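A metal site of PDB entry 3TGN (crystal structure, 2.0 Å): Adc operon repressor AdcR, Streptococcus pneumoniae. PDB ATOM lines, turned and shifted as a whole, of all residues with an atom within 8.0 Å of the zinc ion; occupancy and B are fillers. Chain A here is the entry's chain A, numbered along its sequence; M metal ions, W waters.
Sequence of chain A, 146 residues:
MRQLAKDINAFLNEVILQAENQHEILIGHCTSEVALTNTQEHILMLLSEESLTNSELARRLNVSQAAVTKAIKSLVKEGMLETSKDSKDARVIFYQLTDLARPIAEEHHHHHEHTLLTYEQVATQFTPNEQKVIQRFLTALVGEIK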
ATOM      1  N   LEU A  26      19.625 -14.589  -2.408  1.00  0.00           N
ATOM      2  CA  LEU A  26      19.013 -15.827  -1.947  1.00  0.00           C
ATOM      3  C   LEU A  26      19.123 -15.920  -0.437  1.00  0.00           C
ATOM      4  O   LEU A  26      20.071 -15.393   0.148  1.00  0.00           O
ATOM      5  CB  LEU A  26      19.686 -17.027  -2.615  1.00  0.00           C
ATOM      6  CG  LEU A  26      19.521 -17.125  -4.132  1.00  0.00           C
ATOM      7  CD1 LEU A  26      20.419 -18.210  -4.708  1.00  0.00           C
ATOM      8  CD2 LEU A  26      18.063 -17.363  -4.500  1.00  0.00           C
ATOM      9  N   GLY A  28      19.740 -17.781   3.107  1.00  0.00           N
ATOM     10  CA  GLY A  28      20.434 -18.910   3.687  1.00  0.00           C
ATOM     11  C   GLY A  28      21.608 -19.395   2.849  1.00  0.00           C
ATOM     12  O   GLY A  28      21.909 -18.820   1.799  1.00  0.00           O
ATOM     13  N   HIS A  29      22.261 -20.454   3.307  1.00  0.00           N
ATOM     14  CA  HIS A  29      23.430 -21.010   2.630  1.00  0.00           C
ATOM     15  C   HIS A  29      23.087 -21.755   1.348  1.00  0.00           C
ATOM     16  O   HIS A  29      22.042 -22.404   1.260  1.00  0.00           O
ATOM     17  CB  HIS A  29      24.180 -21.980   3.556  1.00  0.00           C
ATOM     18  CG  HIS A  29      24.787 -21.330   4.762  1.00  0.00           C
ATOM     19  ND1 HIS A  29      24.097 -21.154   5.940  1.00  0.00           N
ATOM     20  CD2 HIS A  29      26.025 -20.818   4.975  1.00  0.00           C
ATOM     21  CE1 HIS A  29      24.885 -20.558   6.823  1.00  0.00           C
ATOM     22  NE2 HIS A  29      26.050 -20.345   6.263  1.00  0.00           N
ATOM     23  N   CYS A  30      23.962 -21.655   0.361  1.00  0.00           N
ATOM     24  CA  CYS A  30      23.968 -22.585  -0.756  1.00  0.00           C
ATOM     25  C   CYS A  30      24.473 -23.910  -0.190  1.00  0.00           C
ATOM     26  O   CYS A  30      25.489 -23.941   0.503  1.00  0.00           O
ATOM     27  CB  CYS A  30      24.900 -22.090  -1.868  1.00  0.00           C
ATOM     28  SG  CYS A  30      25.405 -23.323  -3.099  1.00  0.00           S
ATOM     29  N   THR A  31      23.756 -24.996  -0.455  1.00  0.00           N
ATOM     30  CA  THR A  31      24.154 -26.276   0.102  1.00  0.00           C
ATOM     31  C   THR A  31      24.800 -27.174  -0.937  1.00  0.00           C
ATOM     32  O   THR A  31      24.964 -28.372  -0.719  1.00  0.00           O
ATOM     33  CB  THR A  31      22.974 -27.003   0.765  1.00  0.00           C
ATOM     34  OG1 THR A  31      21.942 -27.229  -0.200  1.00  0.00           O
ATOM     35  CG2 THR A  31      22.427 -26.165   1.928  1.00  0.00           C
ATOM     36  N   SER A  32      25.173 -26.584  -2.066  1.00  0.00           N
ATOM     37  CA  SER A  32      25.952 -27.310  -3.066  1.00  0.00           C
ATOM     38  C   SER A  32      27.325 -27.640  -2.497  1.00  0.00           C
ATOM     39  O   SER A  32      27.950 -26.826  -1.811  1.00  0.00           O
ATOM     40  CB  SER A  32      26.086 -26.478  -4.343  1.00  0.00           C
ATOM     41  OG  SER A  32      26.779 -27.205  -5.338  1.00  0.00           O
ATOM     42  N   GLU A  33      27.801 -28.843  -2.787  1.00  0.00           N
ATOM     43  CA  GLU A  33      29.111 -29.252  -2.314  1.00  0.00           C
ATOM     44  C   GLU A  33      30.170 -28.827  -3.309  1.00  0.00           C
ATOM     45  O   GLU A  33      31.319 -29.275  -3.241  1.00  0.00           O
ATOM     46  CB  GLU A  33      29.131 -30.761  -2.082  1.00  0.00           C
ATOM     47  CG  GLU A  33      28.063 -31.214  -1.088  1.00  0.00           C
ATOM     48  CD  GLU A  33      27.956 -32.713  -0.979  1.00  0.00           C
ATOM     49  OE1 GLU A  33      28.292 -33.415  -1.957  1.00  0.00           O
ATOM     50  OE2 GLU A  33      27.531 -33.194   0.101  1.00  0.00           O
ATOM     51  N   VAL A  34      29.791 -27.932  -4.217  1.00  0.00           N
ATOM     52  CA  VAL A  34      30.677 -27.483  -5.279  1.00  0.00           C
ATOM     53  C   VAL A  34      30.758 -25.955  -5.270  1.00  0.00           C
ATOM     54  O   VAL A  34      29.753 -25.271  -5.091  1.00  0.00           O
ATOM     55  CB  VAL A  34      30.169 -27.968  -6.650  1.00  0.00           C
ATOM     56  CG1 VAL A  34      31.144 -27.585  -7.747  1.00  0.00           C
ATOM     57  CG2 VAL A  34      29.956 -29.480  -6.643  1.00  0.00           C
ATOM     58  N   LEU A  36      30.782 -23.132  -7.125  1.00  0.00           N
ATOM     59  CA  LEU A  36      30.488 -22.327  -8.301  1.00  0.00           C
ATOM     60  C   LEU A  36      29.903 -20.979  -7.863  1.00  0.00           C
ATOM     61  O   LEU A  36      29.353 -20.871  -6.775  1.00  0.00           O
ATOM     62  CB  LEU A  36      29.524 -23.056  -9.231  1.00  0.00           C
ATOM     63  CG  LEU A  36      30.043 -24.354  -9.861  1.00  0.00           C
ATOM     64  CD1 LEU A  36      28.948 -25.064 -10.650  1.00  0.00           C
ATOM     65  CD2 LEU A  36      31.243 -24.069 -10.756  1.00  0.00           C
ATOM     66  N   THR A  37      30.027 -19.959  -8.710  1.00  0.00           N
ATOM     67  CA  THR A  37      29.445 -18.669  -8.396  1.00  0.00           C
ATOM     68  C   THR A  37      27.928 -18.796  -8.469  1.00  0.00           C
ATOM     69  O   THR A  37      27.414 -19.733  -9.070  1.00  0.00           O
ATOM     70  CB  THR A  37      29.905 -17.567  -9.353  1.00  0.00           C
ATOM     71  OG1 THR A  37      29.288 -17.763 -10.641  1.00  0.00           O
ATOM     72  CG2 THR A  37      31.417 -17.574  -9.504  1.00  0.00           C
ATOM     73  N   ASN A  38      27.222 -17.845  -7.856  1.00  0.00           N
ATOM     74  CA  ASN A  38      25.774 -17.893  -7.893  1.00  0.00           C
ATOM     75  C   ASN A  38      25.250 -17.773  -9.315  1.00  0.00           C
ATOM     76  O   ASN A  38      24.281 -18.424  -9.696  1.00  0.00           O
ATOM     77  CB  ASN A  38      25.165 -16.787  -7.023  1.00  0.00           C
ATOM     78  CG  ASN A  38      23.662 -16.902  -6.931  1.00  0.00           C
ATOM     79  OD1 ASN A  38      23.142 -17.694  -6.146  1.00  0.00           O
ATOM     80  ND2 ASN A  38      22.953 -16.121  -7.747  1.00  0.00           N
ATOM     81  N   GLU A  41      25.519 -21.171 -10.994  1.00  0.00           N
ATOM     82  CA  GLU A  41      24.437 -22.045 -10.557  1.00  0.00           C
ATOM     83  C   GLU A  41      23.104 -21.667 -11.203  1.00  0.00           C
ATOM     84  O   GLU A  41      22.349 -22.533 -11.648  1.00  0.00           O
ATOM     85  CB  GLU A  41      24.286 -22.048  -9.038  1.00  0.00           C
ATOM     86  CG  GLU A  41      25.426 -22.743  -8.302  1.00  0.00           C
ATOM     87  CD  GLU A  41      25.036 -23.200  -6.908  1.00  0.00           C
ATOM     88  OE1 GLU A  41      23.886 -22.936  -6.491  1.00  0.00           O
ATOM     89  OE2 GLU A  41      25.873 -23.819  -6.227  1.00  0.00           O
ATOM     90  N   HIS A  42      22.830 -20.368 -11.262  1.00  0.00           N
ATOM     91  CA  HIS A  42      21.581 -19.894 -11.836  1.00  0.00           C
ATOM     92  C   HIS A  42      21.509 -20.256 -13.321  1.00  0.00           C
ATOM     93  O   HIS A  42      20.472 -20.694 -13.819  1.00  0.00           O
ATOM     94  CB  HIS A  42      21.423 -18.379 -11.644  1.00  0.00           C
ATOM     95  CG  HIS A  42      20.030 -17.893 -11.908  1.00  0.00           C
ATOM     96  ND1 HIS A  42      19.076 -17.802 -10.927  1.00  0.00           N
ATOM     97  CD2 HIS A  42      19.437 -17.480 -13.058  1.00  0.00           C
ATOM     98  CE1 HIS A  42      17.948 -17.355 -11.458  1.00  0.00           C
ATOM     99  NE2 HIS A  42      18.140 -17.148 -12.747  1.00  0.00           N
ATOM    100  N   PRO A 103      22.694 -32.199 -10.052  1.00  0.00           N
ATOM    101  CA  PRO A 103      22.363 -31.981  -8.637  1.00  0.00           C
ATOM    102  C   PRO A 103      22.490 -30.509  -8.251  1.00  0.00           C
ATOM    103  O   PRO A 103      21.809 -30.030  -7.350  1.00  0.00           O
ATOM    104  CB  PRO A 103      23.412 -32.817  -7.903  1.00  0.00           C
ATOM    105  CG  PRO A 103      23.901 -33.818  -8.910  1.00  0.00           C
ATOM    106  CD  PRO A 103      23.844 -33.105 -10.222  1.00  0.00           C
ATOM    107  N   ILE A 104      23.377 -29.800  -8.937  1.00  0.00           N
ATOM    108  CA  ILE A 104      23.637 -28.394  -8.668  1.00  0.00           C
ATOM    109  C   ILE A 104      22.458 -27.529  -9.101  1.00  0.00           C
ATOM    110  O   ILE A 104      21.985 -26.676  -8.346  1.00  0.00           O
ATOM    111  CB  ILE A 104      24.927 -27.928  -9.368  1.00  0.00           C
ATOM    112  CG1 ILE A 104      26.091 -28.847  -8.966  1.00  0.00           C
ATOM    113  CG2 ILE A 104      25.218 -26.474  -9.042  1.00  0.00           C
ATOM    114  CD1 ILE A 104      27.422 -28.443  -9.551  1.00  0.00           C
ATOM    115  N   ALA A 105      21.992 -27.748 -10.323  1.00  0.00           N
ATOM    116  CA  ALA A 105      20.800 -27.064 -10.822  1.00  0.00           C
ATOM    117  C   ALA A 105      19.615 -27.324  -9.899  1.00  0.00           C
ATOM    118  O   ALA A 105      18.770 -26.449  -9.685  1.00  0.00           O
ATOM    119  CB  ALA A 105      20.477 -27.514 -12.239  1.00  0.00           C
ATOM    120  N   GLU A 106      19.547 -28.535  -9.346  1.00  0.00           N
ATOM    121  CA  GLU A 106      18.438 -28.888  -8.472  1.00  0.00           C
ATOM    122  C   GLU A 106      18.538 -28.165  -7.137  1.00  0.00           C
ATOM    123  O   GLU A 106      17.550 -27.652  -6.623  1.00  0.00           O
ATOM    124  CB  GLU A 106      18.380 -30.406  -8.273  1.00  0.00           C
ATOM    125  CG  GLU A 106      17.989 -31.151  -9.530  1.00  0.00           C
ATOM    126  CD  GLU A 106      18.382 -32.610  -9.514  1.00  0.00           C
ATOM    127  OE1 GLU A 106      18.902 -33.085  -8.485  1.00  0.00           O
ATOM    128  OE2 GLU A 106      18.170 -33.295 -10.535  1.00  0.00           O
ATOM    129  N   GLU A 107      19.750 -28.109  -6.595  1.00  0.00           N
ATOM    130  CA  GLU A 107      19.993 -27.418  -5.340  1.00  0.00           C
ATOM    131  C   GLU A 107      19.649 -25.943  -5.481  1.00  0.00           C
ATOM    132  O   GLU A 107      19.033 -25.358  -4.591  1.00  0.00           O
ATOM    133  CB  GLU A 107      21.454 -27.572  -4.911  1.00  0.00           C
ATOM    134  CG  GLU A 107      21.788 -26.975  -3.555  1.00  0.00           C
ATOM    135  CD  GLU A 107      22.050 -25.486  -3.598  1.00  0.00           C
ATOM    136  OE1 GLU A 107      22.569 -24.994  -4.625  1.00  0.00           O
ATOM    137  OE2 GLU A 107      21.731 -24.804  -2.611  1.00  0.00           O
ATOM    138  N   HIS A 108      20.039 -25.344  -6.599  1.00  0.00           N
ATOM    139  CA  HIS A 108      19.823 -23.911  -6.818  1.00  0.00           C
ATOM    140  C   HIS A 108      18.341 -23.608  -6.935  1.00  0.00           C
ATOM    141  O   HIS A 108      17.876 -22.547  -6.502  1.00  0.00           O
ATOM    142  CB  HIS A 108      20.571 -23.416  -8.056  1.00  0.00           C
ATOM    143  CG  HIS A 108      20.594 -21.925  -8.183  1.00  0.00           C
ATOM    144  ND1 HIS A 108      21.440 -21.128  -7.460  1.00  0.00           N
ATOM    145  CD2 HIS A 108      19.849 -21.088  -8.957  1.00  0.00           C
ATOM    146  CE1 HIS A 108      21.233 -19.852  -7.777  1.00  0.00           C
ATOM    147  NE2 HIS A 108      20.265 -19.810  -8.677  1.00  0.00           N
ATOM    148  N   HIS A 109      17.587 -24.530  -7.517  1.00  0.00           N
ATOM    149  CA  HIS A 109      16.140 -24.405  -7.602  1.00  0.00           C
ATOM    150  C   HIS A 109      15.512 -24.473  -6.208  1.00  0.00           C
ATOM    151  O   HIS A 109      14.579 -23.735  -5.901  1.00  0.00           O
ATOM    152  CB  HIS A 109      15.559 -25.513  -8.490  1.00  0.00           C
ATOM    153  CG  HIS A 109      14.065 -25.507  -8.562  1.00  0.00           C
ATOM    154  ND1 HIS A 109      13.365 -24.589  -9.315  1.00  0.00           N
ATOM    155  CD2 HIS A 109      13.138 -26.297  -7.970  1.00  0.00           C
ATOM    156  CE1 HIS A 109      12.068 -24.827  -9.187  1.00  0.00           C
ATOM    157  NE2 HIS A 109      11.908 -25.856  -8.384  1.00  0.00           N
ATOM    158  N   HIS A 110      16.020 -25.380  -5.374  1.00  0.00           N
ATOM    159  CA  HIS A 110      15.494 -25.527  -4.026  1.00  0.00           C
ATOM    160  C   HIS A 110      15.829 -24.303  -3.188  1.00  0.00           C
ATOM    161  O   HIS A 110      15.039 -23.891  -2.328  1.00  0.00           O
ATOM    162  CB  HIS A 110      16.060 -26.786  -3.351  1.00  0.00           C
ATOM    163  CG  HIS A 110      15.533 -28.055  -3.947  1.00  0.00           C
ATOM    164  ND1 HIS A 110      14.189 -28.308  -4.109  1.00  0.00           N
ATOM    165  CD2 HIS A 110      16.183 -29.141  -4.431  1.00  0.00           C
ATOM    166  CE1 HIS A 110      14.027 -29.494  -4.662  1.00  0.00           C
ATOM    167  NE2 HIS A 110      15.221 -30.018  -4.867  1.00  0.00           N
ATOM    168  N   HIS A 111      16.987 -23.721  -3.460  1.00  0.00           N
ATOM    169  CA  HIS A 111      17.409 -22.509  -2.774  1.00  0.00           C
ATOM    170  C   HIS A 111      16.433 -21.387  -3.095  1.00  0.00           C
ATOM    171  O   HIS A 111      16.021 -20.641  -2.211  1.00  0.00           O
ATOM    172  CB  HIS A 111      18.828 -22.132  -3.199  1.00  0.00           C
ATOM    173  CG  HIS A 111      19.561 -21.303  -2.199  1.00  0.00           C
ATOM    174  ND1 HIS A 111      20.883 -20.938  -2.349  1.00  0.00           N
ATOM    175  CD2 HIS A 111      19.165 -20.780  -1.008  1.00  0.00           C
ATOM    176  CE1 HIS A 111      21.261 -20.220  -1.318  1.00  0.00           C
ATOM    177  NE2 HIS A 111      20.243 -20.109  -0.488  1.00  0.00           N
ATOM    178  N   HIS A 112      16.038 -21.292  -4.365  1.00  0.00           N
ATOM    179  CA  HIS A 112      15.032 -20.316  -4.775  1.00  0.00           C
ATOM    180  C   HIS A 112      13.691 -20.547  -4.076  1.00  0.00           C
ATOM    181  O   HIS A 112      13.035 -19.601  -3.641  1.00  0.00           O
ATOM    182  CB  HIS A 112      14.841 -20.330  -6.292  1.00  0.00           C
ATOM    183  CG  HIS A 112      15.757 -19.406  -7.021  1.00  0.00           C
ATOM    184  ND1 HIS A 112      15.419 -18.107  -7.328  1.00  0.00           N
ATOM    185  CD2 HIS A 112      17.008 -19.583  -7.494  1.00  0.00           C
ATOM    186  CE1 HIS A 112      16.416 -17.528  -7.965  1.00  0.00           C
ATOM    187  NE2 HIS A 112      17.395 -18.399  -8.085  1.00  0.00           N
HETATM  188 ZN    ZN M   1      23.619 -23.300  -4.532  1.00  0.00          ZN
HETATM  189  O   HOH W   1      22.440 -21.581  -4.439  1.00  0.00           O
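N of Thr 31 sits at hydrogen-bond distance from OE2 of Glu 107, 3.0 Å away. OE1 of Glu 41 sits close to ND1 of His 108, at 3.2 Å. The side-chain sulfur (SG) of Cys 30 lies close to the backbone NH (N) of Ser 32, 3.4 Å away.
Water W1 lies within hydrogen-bond range of ND1 of His 111 (2.7 Å) and ND1 of His 108 (3.2 Å).
Of the 23 residues printed, 3 come within 4 Å of the zinc ion. Along chain A the residues within 4 Å of the zinc ion span positions 30 to 107.
The zinc ion is bound by OE1 of Glu 107, at 2.0 Å. The zinc ion is bound by the side-chain carboxylate (OE1) of Glu 41 (2.0 Å). Water W1 binds the zinc ion (2.1 Å). SG of Cys 30 is bound to the zinc ion, 2.3 Å away. The zinc ion has four donor atoms within binding distance.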
